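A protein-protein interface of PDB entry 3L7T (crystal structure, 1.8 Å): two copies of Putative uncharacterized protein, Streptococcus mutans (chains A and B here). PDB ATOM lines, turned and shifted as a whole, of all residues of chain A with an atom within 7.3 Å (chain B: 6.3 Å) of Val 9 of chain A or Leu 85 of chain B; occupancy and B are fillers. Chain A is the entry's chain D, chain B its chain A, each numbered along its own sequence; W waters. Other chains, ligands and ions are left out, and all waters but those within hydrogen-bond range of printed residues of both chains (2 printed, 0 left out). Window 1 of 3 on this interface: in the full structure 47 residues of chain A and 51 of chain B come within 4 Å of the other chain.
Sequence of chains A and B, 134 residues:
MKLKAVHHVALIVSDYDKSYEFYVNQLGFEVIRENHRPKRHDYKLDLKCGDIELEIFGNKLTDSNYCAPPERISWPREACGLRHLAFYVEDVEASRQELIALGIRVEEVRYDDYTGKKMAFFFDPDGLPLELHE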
ATOM      1  N   VAL A   6      13.346  19.346 -31.514  1.00  0.00           N
ATOM      2  CA  VAL A   6      12.037  19.068 -30.970  1.00  0.00           C
ATOM      3  C   VAL A   6      11.185  20.309 -31.109  1.00  0.00           C
ATOM      4  O   VAL A   6      11.635  21.429 -30.850  1.00  0.00           O
ATOM      5  CB  VAL A   6      12.098  18.616 -29.484  1.00  0.00           C
ATOM      6  CG1 VAL A   6      10.702  18.494 -28.874  1.00  0.00           C
ATOM      7  CG2 VAL A   6      12.811  17.271 -29.387  1.00  0.00           C
ATOM      8  N   HIS A   7       9.925  20.099 -31.436  1.00  0.00           N
ATOM      9  CA  HIS A   7       9.012  21.227 -31.582  1.00  0.00           C
ATOM     10  C   HIS A   7       8.220  21.382 -30.309  1.00  0.00           C
ATOM     11  O   HIS A   7       8.095  22.479 -29.763  1.00  0.00           O
ATOM     12  CB  HIS A   7       8.079  20.976 -32.751  1.00  0.00           C
ATOM     13  CG  HIS A   7       7.127  22.098 -33.006  1.00  0.00           C
ATOM     14  ND1 HIS A   7       5.873  22.153 -32.438  1.00  0.00           N
ATOM     15  CD2 HIS A   7       7.265  23.227 -33.742  1.00  0.00           C
ATOM     16  CE1 HIS A   7       5.271  23.266 -32.831  1.00  0.00           C
ATOM     17  NE2 HIS A   7       6.087  23.922 -33.639  1.00  0.00           N
ATOM     18  N   HIS A   8       7.697  20.267 -29.811  1.00  0.00           N
ATOM     19  CA  HIS A   8       7.007  20.258 -28.535  1.00  0.00           C
ATOM     20  C   HIS A   8       6.901  18.835 -28.014  1.00  0.00           C
ATOM     21  O   HIS A   8       7.133  17.886 -28.746  1.00  0.00           O
ATOM     22  CB  HIS A   8       5.598  20.879 -28.634  1.00  0.00           C
ATOM     23  CG  HIS A   8       4.636  20.096 -29.484  1.00  0.00           C
ATOM     24  ND1 HIS A   8       4.441  20.357 -30.822  1.00  0.00           N
ATOM     25  CD2 HIS A   8       3.791  19.086 -29.175  1.00  0.00           C
ATOM     26  CE1 HIS A   8       3.551  19.514 -31.312  1.00  0.00           C
ATOM     27  NE2 HIS A   8       3.148  18.726 -30.338  1.00  0.00           N
ATOM     28  N   VAL A   9       6.650  18.735 -26.722  1.00  0.00           N
ATOM     29  CA  VAL A   9       6.405  17.471 -26.042  1.00  0.00           C
ATOM     30  C   VAL A   9       5.028  17.599 -25.399  1.00  0.00           C
ATOM     31  O   VAL A   9       4.703  18.619 -24.776  1.00  0.00           O
ATOM     32  CB  VAL A   9       7.407  17.278 -24.919  1.00  0.00           C
ATOM     33  CG1 VAL A   9       7.085  16.014 -24.089  1.00  0.00           C
ATOM     34  CG2 VAL A   9       8.820  17.189 -25.473  1.00  0.00           C
ATOM     35  N   ALA A  10       4.188  16.593 -25.586  1.00  0.00           N
ATOM     36  CA  ALA A  10       2.861  16.646 -25.011  1.00  0.00           C
ATOM     37  C   ALA A  10       2.715  15.674 -23.854  1.00  0.00           C
ATOM     38  O   ALA A  10       3.407  14.629 -23.787  1.00  0.00           O
ATOM     39  CB  ALA A  10       1.781  16.408 -26.093  1.00  0.00           C
ATOM     40  N   LEU A  11       1.821  16.012 -22.939  1.00  0.00           N
ATOM     41  CA  LEU A  11       1.528  15.147 -21.816  1.00  0.00           C
ATOM     42  C   LEU A  11       0.070  15.216 -21.409  1.00  0.00           C
ATOM     43  O   LEU A  11      -0.631  16.206 -21.711  1.00  0.00           O
ATOM     44  CB  LEU A  11       2.451  15.438 -20.638  1.00  0.00           C
ATOM     45  CG  LEU A  11       2.337  16.783 -19.934  1.00  0.00           C
ATOM     46  CD1 LEU A  11       1.535  16.562 -18.650  1.00  0.00           C
ATOM     47  CD2 LEU A  11       3.738  17.279 -19.567  1.00  0.00           C
ATOM     48  N   LEU A  45      -3.044  23.261 -22.927  1.00  0.00           N
ATOM     49  CA  LEU A  45      -2.262  24.300 -22.262  1.00  0.00           C
ATOM     50  C   LEU A  45      -0.835  24.267 -22.807  1.00  0.00           C
ATOM     51  O   LEU A  45      -0.151  23.243 -22.702  1.00  0.00           O
ATOM     52  CB  LEU A  45      -2.272  24.091 -20.747  1.00  0.00           C
ATOM     53  CG  LEU A  45      -1.409  25.038 -19.899  1.00  0.00           C
ATOM     54  CD1 LEU A  45      -2.037  26.458 -19.855  1.00  0.00           C
ATOM     55  CD2 LEU A  45      -1.184  24.512 -18.482  1.00  0.00           C
ATOM     56  N   LEU A  47       2.915  25.656 -22.865  1.00  0.00           N
ATOM     57  CA  LEU A  47       3.929  26.298 -22.013  1.00  0.00           C
ATOM     58  C   LEU A  47       5.257  26.437 -22.742  1.00  0.00           C
ATOM     59  O   LEU A  47       5.656  25.550 -23.498  1.00  0.00           O
ATOM     60  CB  LEU A  47       4.152  25.470 -20.746  1.00  0.00           C
ATOM     61  CG  LEU A  47       2.883  25.184 -19.940  1.00  0.00           C
ATOM     62  CD1 LEU A  47       3.202  24.351 -18.735  1.00  0.00           C
ATOM     63  CD2 LEU A  47       2.183  26.501 -19.518  1.00  0.00           C
ATOM     64  N   ILE A  52      11.313  24.996 -27.020  1.00  0.00           N
ATOM     65  CA  ILE A  52      10.224  24.092 -27.346  1.00  0.00           C
ATOM     66  C   ILE A  52       8.986  24.446 -26.541  1.00  0.00           C
ATOM     67  O   ILE A  52       9.061  25.236 -25.603  1.00  0.00           O
ATOM     68  CB  ILE A  52      10.611  22.625 -27.135  1.00  0.00           C
ATOM     69  CG1 ILE A  52      10.440  22.201 -25.687  1.00  0.00           C
ATOM     70  CG2 ILE A  52      12.027  22.331 -27.651  1.00  0.00           C
ATOM     71  CD1 ILE A  52      10.313  20.678 -25.574  1.00  0.00           C
ATOM     72  N   GLU A  53       7.853  23.857 -26.897  1.00  0.00           N
ATOM     73  CA  GLU A  53       6.639  24.025 -26.132  1.00  0.00           C
ATOM     74  C   GLU A  53       6.318  22.735 -25.387  1.00  0.00           C
ATOM     75  O   GLU A  53       6.707  21.667 -25.842  1.00  0.00           O
ATOM     76  CB  GLU A  53       5.479  24.383 -27.059  1.00  0.00           C
ATOM     77  CG  GLU A  53       5.628  25.709 -27.804  1.00  0.00           C
ATOM     78  CD  GLU A  53       4.296  26.241 -28.330  1.00  0.00           C
ATOM     79  OE1 GLU A  53       3.256  25.564 -28.165  1.00  0.00           O
ATOM     80  OE2 GLU A  53       4.279  27.354 -28.894  1.00  0.00           O
ATOM     81  N   LEU A  54       5.742  22.856 -24.193  1.00  0.00           N
ATOM     82  CA  LEU A  54       5.126  21.720 -23.496  1.00  0.00           C
ATOM     83  C   LEU A  54       3.617  21.851 -23.636  1.00  0.00           C
ATOM     84  O   LEU A  54       3.044  22.892 -23.281  1.00  0.00           O
ATOM     85  CB  LEU A  54       5.473  21.730 -22.003  1.00  0.00           C
ATOM     86  CG  LEU A  54       6.953  21.832 -21.604  1.00  0.00           C
ATOM     87  CD1 LEU A  54       7.132  21.936 -20.071  1.00  0.00           C
ATOM     88  CD2 LEU A  54       7.738  20.645 -22.155  1.00  0.00           C
ATOM     89  N   GLU A  55       2.972  20.821 -24.171  1.00  0.00           N
ATOM     90  CA  GLU A  55       1.532  20.856 -24.325  1.00  0.00           C
ATOM     91  C   GLU A  55       0.936  19.956 -23.273  1.00  0.00           C
ATOM     92  O   GLU A  55       1.183  18.737 -23.248  1.00  0.00           O
ATOM     93  CB  GLU A  55       1.068  20.379 -25.701  1.00  0.00           C
ATOM     94  CG  GLU A  55       1.708  21.011 -26.895  1.00  0.00           C
ATOM     95  CD  GLU A  55       1.019  20.623 -28.214  1.00  0.00           C
ATOM     96  OE1 GLU A  55       0.429  19.517 -28.330  1.00  0.00           O
ATOM     97  OE2 GLU A  55       1.093  21.431 -29.158  1.00  0.00           O
ATOM     98  N   ILE A  56       0.161  20.557 -22.394  1.00  0.00           N
ATOM     99  CA  ILE A  56      -0.499  19.821 -21.368  1.00  0.00           C
ATOM    100  C   ILE A  56      -1.969  19.656 -21.700  1.00  0.00           C
ATOM    101  O   ILE A  56      -2.672  20.647 -21.963  1.00  0.00           O
ATOM    102  CB  ILE A  56      -0.295  20.506 -20.036  1.00  0.00           C
ATOM    103  CG1 ILE A  56       1.206  20.653 -19.774  1.00  0.00           C
ATOM    104  CG2 ILE A  56      -1.035  19.786 -18.942  1.00  0.00           C
ATOM    105  CD1 ILE A  56       1.529  20.941 -18.349  1.00  0.00           C
ATOM    106  N   PHE A  57      -2.420  18.402 -21.738  1.00  0.00           N
ATOM    107  CA  PHE A  57      -3.809  18.089 -22.093  1.00  0.00           C
ATOM    108  C   PHE A  57      -4.532  17.548 -20.884  1.00  0.00           C
ATOM    109  O   PHE A  57      -4.072  16.621 -20.221  1.00  0.00           O
ATOM    110  CB  PHE A  57      -3.877  17.028 -23.193  1.00  0.00           C
ATOM    111  CG  PHE A  57      -3.370  17.479 -24.523  1.00  0.00           C
ATOM    112  CD1 PHE A  57      -4.245  18.012 -25.467  1.00  0.00           C
ATOM    113  CD2 PHE A  57      -2.029  17.363 -24.853  1.00  0.00           C
ATOM    114  CE1 PHE A  57      -3.813  18.339 -26.733  1.00  0.00           C
ATOM    115  CE2 PHE A  57      -1.582  17.714 -26.121  1.00  0.00           C
ATOM    116  CZ  PHE A  57      -2.468  18.208 -27.055  1.00  0.00           C
ATOM    117  N   LEU A  82       6.784   7.311 -24.177  1.00  0.00           N
ATOM    118  CA  LEU A  82       7.593   8.326 -23.516  1.00  0.00           C
ATOM    119  C   LEU A  82       7.581   8.109 -22.012  1.00  0.00           C
ATOM    120  O   LEU A  82       6.537   7.794 -21.415  1.00  0.00           O
ATOM    121  CB  LEU A  82       7.048   9.719 -23.847  1.00  0.00           C
ATOM    122  CG  LEU A  82       7.233  10.072 -25.313  1.00  0.00           C
ATOM    123  CD1 LEU A  82       6.408  11.332 -25.586  1.00  0.00           C
ATOM    124  CD2 LEU A  82       8.692  10.288 -25.681  1.00  0.00           C
ATOM    125  N   HIS A  84      10.082   9.755 -19.314  1.00  0.00           N
ATOM    126  CA  HIS A  84      10.202  10.910 -18.401  1.00  0.00           C
ATOM    127  C   HIS A  84      10.921  12.061 -19.077  1.00  0.00           C
ATOM    128  O   HIS A  84      11.345  11.935 -20.209  1.00  0.00           O
ATOM    129  CB  HIS A  84      10.924  10.549 -17.101  1.00  0.00           C
ATOM    130  CG  HIS A  84      12.360  10.168 -17.287  1.00  0.00           C
ATOM    131  ND1 HIS A  84      12.829   8.903 -17.014  1.00  0.00           N
ATOM    132  CD2 HIS A  84      13.437  10.894 -17.663  1.00  0.00           C
ATOM    133  CE1 HIS A  84      14.122   8.850 -17.265  1.00  0.00           C
ATOM    134  NE2 HIS A  84      14.511  10.038 -17.689  1.00  0.00           N
ATOM    135  N   LEU A  85      10.840  13.229 -18.456  1.00  0.00           N
ATOM    136  CA  LEU A  85      11.281  14.471 -19.060  1.00  0.00           C
ATOM    137  C   LEU A  85      12.229  15.143 -18.086  1.00  0.00           C
ATOM    138  O   LEU A  85      11.939  15.235 -16.886  1.00  0.00           O
ATOM    139  CB  LEU A  85      10.042  15.355 -19.281  1.00  0.00           C
ATOM    140  CG  LEU A  85      10.236  16.679 -20.005  1.00  0.00           C
ATOM    141  CD1 LEU A  85      10.785  16.494 -21.395  1.00  0.00           C
ATOM    142  CD2 LEU A  85       8.864  17.382 -20.096  1.00  0.00           C
ATOM    143  N   VAL B   6      14.550  21.910 -21.921  1.00  0.00           N
ATOM    144  CA  VAL B   6      14.568  20.464 -21.773  1.00  0.00           C
ATOM    145  C   VAL B   6      15.999  19.991 -21.983  1.00  0.00           C
ATOM    146  O   VAL B   6      16.669  20.412 -22.930  1.00  0.00           O
ATOM    147  CB  VAL B   6      13.613  19.794 -22.783  1.00  0.00           C
ATOM    148  CG1 VAL B   6      13.786  18.290 -22.755  1.00  0.00           C
ATOM    149  CG2 VAL B   6      12.196  20.137 -22.401  1.00  0.00           C
ATOM    150  N   VAL B   9      14.582  13.747 -23.187  1.00  0.00           N
ATOM    151  CA  VAL B   9      13.298  13.062 -23.095  1.00  0.00           C
ATOM    152  C   VAL B   9      13.659  11.597 -23.226  1.00  0.00           C
ATOM    153  O   VAL B   9      14.480  11.245 -24.076  1.00  0.00           O
ATOM    154  CB  VAL B   9      12.410  13.411 -24.301  1.00  0.00           C
ATOM    155  CG1 VAL B   9      10.994  12.874 -24.066  1.00  0.00           C
ATOM    156  CG2 VAL B   9      12.321  14.945 -24.446  1.00  0.00           C
ATOM    157  N   LEU B  11      12.420   7.421 -23.391  1.00  0.00           N
ATOM    158  CA  LEU B  11      11.306   6.589 -23.801  1.00  0.00           C
ATOM    159  C   LEU B  11      11.732   5.163 -23.706  1.00  0.00           C
ATOM    160  O   LEU B  11      12.940   4.862 -23.662  1.00  0.00           O
ATOM    161  CB  LEU B  11      10.863   6.937 -25.219  1.00  0.00           C
ATOM    162  CG  LEU B  11      11.840   6.770 -26.375  1.00  0.00           C
ATOM    163  CD1 LEU B  11      11.555   5.448 -27.051  1.00  0.00           C
ATOM    164  CD2 LEU B  11      11.661   7.900 -27.380  1.00  0.00           C
ATOM    165  N   LEU B  54      17.589  12.430 -26.829  1.00  0.00           N
ATOM    166  CA  LEU B  54      16.532  11.415 -26.653  1.00  0.00           C
ATOM    167  C   LEU B  54      17.192  10.197 -26.046  1.00  0.00           C
ATOM    168  O   LEU B  54      18.188   9.722 -26.582  1.00  0.00           O
ATOM    169  CB  LEU B  54      15.964  11.016 -28.025  1.00  0.00           C
ATOM    170  CG  LEU B  54      15.461  12.173 -28.860  1.00  0.00           C
ATOM    171  CD1 LEU B  54      14.906  11.605 -30.208  1.00  0.00           C
ATOM    172  CD2 LEU B  54      14.423  12.974 -28.135  1.00  0.00           C
ATOM    173  N   LEU B  82       3.642  11.323 -20.212  1.00  0.00           N
ATOM    174  CA  LEU B  82       4.045  11.830 -21.508  1.00  0.00           C
ATOM    175  C   LEU B  82       3.399  11.124 -22.678  1.00  0.00           C
ATOM    176  O   LEU B  82       3.329   9.894 -22.717  1.00  0.00           O
ATOM    177  CB  LEU B  82       5.557  11.799 -21.649  1.00  0.00           C
ATOM    178  CG  LEU B  82       6.290  12.646 -20.631  1.00  0.00           C
ATOM    179  CD1 LEU B  82       7.744  12.153 -20.513  1.00  0.00           C
ATOM    180  CD2 LEU B  82       6.280  14.099 -21.096  1.00  0.00           C
ATOM    181  N   ARG B  83       2.892  11.915 -23.611  1.00  0.00           N
ATOM    182  CA  ARG B  83       1.948  11.458 -24.613  1.00  0.00           C
ATOM    183  C   ARG B  83       2.636  11.254 -25.955  1.00  0.00           C
ATOM    184  O   ARG B  83       2.648  10.141 -26.489  1.00  0.00           O
ATOM    185  CB  ARG B  83       0.814  12.496 -24.753  1.00  0.00           C
ATOM    186  CG  ARG B  83      -0.327  12.062 -25.642  1.00  0.00           C
ATOM    187  CD  ARG B  83      -1.315  13.223 -25.855  1.00  0.00           C
ATOM    188  NE  ARG B  83      -2.385  12.777 -26.734  1.00  0.00           N
ATOM    189  CZ  ARG B  83      -3.276  13.565 -27.333  1.00  0.00           C
ATOM    190  NH1 ARG B  83      -3.297  14.879 -27.113  1.00  0.00           N
ATOM    191  NH2 ARG B  83      -4.172  13.018 -28.148  1.00  0.00           N
ATOM    192  N   HIS B  84       3.154  12.341 -26.534  1.00  0.00           N
ATOM    193  CA  HIS B  84       3.799  12.283 -27.837  1.00  0.00           C
ATOM    194  C   HIS B  84       4.865  13.363 -27.961  1.00  0.00           C
ATOM    195  O   HIS B  84       5.049  14.181 -27.059  1.00  0.00           O
ATOM    196  CB  HIS B  84       2.782  12.339 -28.989  1.00  0.00           C
ATOM    197  CG  HIS B  84       2.206  13.700 -29.248  1.00  0.00           C
ATOM    198  ND1 HIS B  84       0.898  14.023 -28.954  1.00  0.00           N
ATOM    199  CD2 HIS B  84       2.733  14.792 -29.854  1.00  0.00           C
ATOM    200  CE1 HIS B  84       0.660  15.270 -29.325  1.00  0.00           C
ATOM    201  NE2 HIS B  84       1.772  15.770 -29.837  1.00  0.00           N
ATOM    202  N   LEU B  85       5.624  13.288 -29.039  1.00  0.00           N
ATOM    203  CA  LEU B  85       6.787  14.120 -29.235  1.00  0.00           C
ATOM    204  C   LEU B  85       6.732  14.594 -30.662  1.00  0.00           C
ATOM    205  O   LEU B  85       6.446  13.821 -31.581  1.00  0.00           O
ATOM    206  CB  LEU B  85       8.052  13.264 -28.989  1.00  0.00           C
ATOM    207  CG  LEU B  85       9.440  13.801 -29.258  1.00  0.00           C
ATOM    208  CD1 LEU B  85       9.672  15.001 -28.407  1.00  0.00           C
ATOM    209  CD2 LEU B  85      10.465  12.712 -28.902  1.00  0.00           C
ATOM    210  N   ALA B  86       6.987  15.885 -30.864  1.00  0.00           N
ATOM    211  CA  ALA B  86       6.911  16.456 -32.192  1.00  0.00           C
ATOM    212  C   ALA B  86       8.251  17.035 -32.555  1.00  0.00           C
ATOM    213  O   ALA B  86       8.932  17.585 -31.690  1.00  0.00           O
ATOM    214  CB  ALA B  86       5.850  17.579 -32.215  1.00  0.00           C
ATOM    215  N   PHE B  87       8.610  16.945 -33.839  1.00  0.00           N
ATOM    216  CA  PHE B  87       9.877  17.458 -34.327  1.00  0.00           C
ATOM    217  C   PHE B  87       9.615  18.566 -35.326  1.00  0.00           C
ATOM    218  O   PHE B  87       8.731  18.447 -36.183  1.00  0.00           O
ATOM    219  CB  PHE B  87      10.649  16.343 -35.055  1.00  0.00           C
ATOM    220  CG  PHE B  87      10.951  15.175 -34.193  1.00  0.00           C
ATOM    221  CD1 PHE B  87      11.953  15.264 -33.221  1.00  0.00           C
ATOM    222  CD2 PHE B  87      10.212  13.993 -34.307  1.00  0.00           C
ATOM    223  CE1 PHE B  87      12.222  14.186 -32.368  1.00  0.00           C
ATOM    224  CE2 PHE B  87      10.467  12.908 -33.456  1.00  0.00           C
ATOM    225  CZ  PHE B  87      11.481  13.006 -32.486  1.00  0.00           C
ATOM    226  N   PHE B 121       1.310  13.119 -38.264  1.00  0.00           N
ATOM    227  CA  PHE B 121       1.713  12.038 -37.362  1.00  0.00           C
ATOM    228  C   PHE B 121       2.219  10.782 -38.047  1.00  0.00           C
ATOM    229  O   PHE B 121       1.677  10.321 -39.071  1.00  0.00           O
ATOM    230  CB  PHE B 121       0.570  11.643 -36.423  1.00  0.00           C
ATOM    231  CG  PHE B 121       0.336  12.618 -35.298  1.00  0.00           C
ATOM    232  CD1 PHE B 121       1.053  12.514 -34.104  1.00  0.00           C
ATOM    233  CD2 PHE B 121      -0.624  13.609 -35.423  1.00  0.00           C
ATOM    234  CE1 PHE B 121       0.825  13.399 -33.058  1.00  0.00           C
ATOM    235  CE2 PHE B 121      -0.861  14.498 -34.390  1.00  0.00           C
ATOM    236  CZ  PHE B 121      -0.132  14.401 -33.208  1.00  0.00           C
ATOM    237  N   LEU B 128       4.344   4.664 -30.493  1.00  0.00           N
ATOM    238  CA  LEU B 128       4.529   5.987 -29.851  1.00  0.00           C
ATOM    239  C   LEU B 128       4.231   7.041 -30.941  1.00  0.00           C
ATOM    240  O   LEU B 128       4.862   7.017 -32.003  1.00  0.00           O
ATOM    241  CB  LEU B 128       5.984   6.125 -29.415  1.00  0.00           C
ATOM    242  CG  LEU B 128       6.371   7.494 -28.830  1.00  0.00           C
ATOM    243  CD1 LEU B 128       5.452   7.743 -27.644  1.00  0.00           C
ATOM    244  CD2 LEU B 128       7.857   7.483 -28.418  1.00  0.00           C
ATOM    245  N   PRO B 129       3.249   7.932 -30.710  1.00  0.00           N
ATOM    246  CA  PRO B 129       2.985   8.942 -31.754  1.00  0.00           C
ATOM    247  C   PRO B 129       4.109   9.996 -31.843  1.00  0.00           C
ATOM    248  O   PRO B 129       4.508  10.577 -30.818  1.00  0.00           O
ATOM    249  CB  PRO B 129       1.688   9.621 -31.294  1.00  0.00           C
ATOM    250  CG  PRO B 129       1.046   8.672 -30.317  1.00  0.00           C
ATOM    251  CD  PRO B 129       2.263   7.980 -29.628  1.00  0.00           C
ATOM    252  N   LEU B 130       4.623  10.189 -33.050  1.00  0.00           N
ATOM    253  CA  LEU B 130       5.639  11.180 -33.350  1.00  0.00           C
ATOM    254  C   LEU B 130       5.085  12.110 -34.418  1.00  0.00           C
ATOM    255  O   LEU B 130       4.240  11.718 -35.214  1.00  0.00           O
ATOM    256  CB  LEU B 130       6.934  10.522 -33.859  1.00  0.00           C
ATOM    257  CG  LEU B 130       7.521   9.452 -32.944  1.00  0.00           C
ATOM    258  CD1 LEU B 130       8.709   8.703 -33.596  1.00  0.00           C
ATOM    259  CD2 LEU B 130       7.908  10.065 -31.539  1.00  0.00           C
ATOM    260  N   GLU B 131       5.524  13.358 -34.422  1.00  0.00           N
ATOM    261  CA  GLU B 131       4.829  14.336 -35.246  1.00  0.00           C
ATOM    262  C   GLU B 131       5.866  15.162 -35.964  1.00  0.00           C
ATOM    263  O   GLU B 131       6.926  15.440 -35.384  1.00  0.00           O
ATOM    264  CB  GLU B 131       3.950  15.204 -34.339  1.00  0.00           C
ATOM    265  CG  GLU B 131       3.106  16.216 -35.032  1.00  0.00           C
ATOM    266  CD  GLU B 131       2.508  17.244 -34.063  1.00  0.00           C
ATOM    267  OE1 GLU B 131       2.202  16.908 -32.895  1.00  0.00           O
ATOM    268  OE2 GLU B 131       2.358  18.407 -34.480  1.00  0.00           O
ATOM    269  N   LEU B 132       5.644  15.401 -37.260  1.00  0.00           N
ATOM    270  CA  LEU B 132       6.442  16.368 -38.049  1.00  0.00           C
ATOM    271  C   LEU B 132       5.689  17.684 -38.015  1.00  0.00           C
ATOM    272  O   LEU B 132       4.460  17.689 -38.152  1.00  0.00           O
ATOM    273  CB  LEU B 132       6.493  15.908 -39.504  1.00  0.00           C
ATOM    274  CG  LEU B 132       7.070  14.507 -39.728  1.00  0.00           C
ATOM    275  CD1 LEU B 132       6.962  14.128 -41.195  1.00  0.00           C
ATOM    276  CD2 LEU B 132       8.518  14.544 -39.236  1.00  0.00           C
HETATM  277  O   HOH W   1       3.821   7.576 -24.269  1.00  0.00           O
HETATM  278  O   HOH W   2       5.062   9.040 -18.971  1.00  0.00           O
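The backbone NH (N) of Leu 85 of chain B lies within hydrogen-bond range of the backbone carbonyl oxygen (O) of Pro 129 of chain B, at 3.4 Å.
NE2 of His 84 of chain B sits at hydrogen-bond distance from OE1 of Glu 131 of chain B (3.3 Å).
O of His 7 of chain A is in hydrogen-bond range of N of Glu 53 of chain A, 3.2 Å away.
The backbone carbonyl oxygen of Val 9 of chain A sits at hydrogen-bond distance from the backbone NH of Glu 55 of chain A (2.9 Å).
The backbone NH of Phe 87 of chain B is in hydrogen-bond range of the backbone carbonyl oxygen of Glu 131 of chain B.
N of Val 9 of chain A sits at hydrogen-bond distance from O of Glu 53 of chain A, 3.1 Å away.
Leu 85 of chain B touches Val 6 of chain A.
Val 6 of chain A touches Ala 86 of chain B (CG1 to O, 3.4 Å).
CA of Leu 85 of chain B touches O of His 8 of chain A (3.8 Å).
Ala 10 of chain A touches Leu 82 of chain B.
Phe 57 of chain A touches Arg 83 of chain B.
CD2 of Leu 82 of chain A touches CG1 of Val 9 of chain B, 3.8 Å away.
CB of Leu 82 of chain A touches CB of Leu 82 of chain B (3.4 Å).
Leu 82 of chain A touches Arg 83 of chain B (CD1 to C, 3.8 Å).
CD1 of Leu 82 of chain A touches O of His 84 of chain B, 3.5 Å away.
Leu 82 of chain A touches Leu 128 of chain B (N to CD1, 3.7 Å).
Of the printed residues of chain B, Val 6 of chain A touches Leu 85 (3.7 Å) and Ala 86 (3.4 Å).
Val 9 of chain A touches three residues of chain B.
Printed residues of chain B within 4 Å of Leu 11 of chain A: Arg 83 (3.9 Å).
Leu 85 of chain B touches just these residues of chain A: Val 6 (3.7 Å), His 8 (3.8 Å) and Val 9 (3.8 Å).
Of the printed residues of chain A, Ala 86 of chain B touches Val 6, His 7 and His 8.
The nearest printed residue of chain B that does not touch His 8 of chain A is Phe 87 of chain B (5.3 Å).
Water W1 lies within hydrogen-bond range of the backbone carbonyl oxygen (O) of Leu 82 of chain B (2.8 Å) and the backbone NH (N) of Leu 82 of chain A (3.0 Å).
Water W2 lies within hydrogen-bond range of the backbone NH (N) of Leu 82 of chain B and the backbone carbonyl oxygen (O) of Leu 82 of chain A.
Val 9 of chain A touches Leu 82 of chain B, and with the chains exchanged Leu 82 of chain A touches Val 9 of chain B.
Val 9 of chain A touches Leu 85 of chain B, and with the chains exchanged Leu 85 of chain A touches Val 9 of chain B.
Leu 82 of chain A touches Leu 11 of chain B, but with the chains exchanged Leu 11 of chain A does not touch Leu 82 of chain B (4.04 Å).
Leu 82 of chain A touches His 84 of chain B, and with the chains exchanged His 84 of chain A touches Leu 82 of chain B.
Of the 28 pairs that touch across the chains among the printed residues, 11 have their exchanged pair printed and touching as well.
Of the 17 printed residues of chain A, 11 touch a printed residue of chain B.
Of the 16 printed residues of chain B, 11 touch a printed residue of chain A.
Among the printed residues, 28 pairs touch across the chains.
O of Ala 10 of chain A lies within hydrogen-bond range of N of Arg 83 of chain B, at 2.8 Å.
A ring nitrogen (NE2) of His 8 of chain A is in hydrogen-bond range of a ring nitrogen (NE2) of His 84 of chain B, at 3.3 Å.
The backbone NH of Ala 86 of chain B lies within hydrogen-bond range of the backbone carbonyl oxygen of His 8 of chain A (2.9 Å).
N of His 7 of chain A sits at hydrogen-bond distance from O of Ala 86 of chain B.
The backbone carbonyl oxygen of His 84 of chain B sits at hydrogen-bond distance from the backbone NH of Ala 10 of chain A, at 3.0 Å.
A ring nitrogen (NE2) of His 8 of chain A sits at hydrogen-bond distance from the side-chain carboxylate of Glu 131 of chain B.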
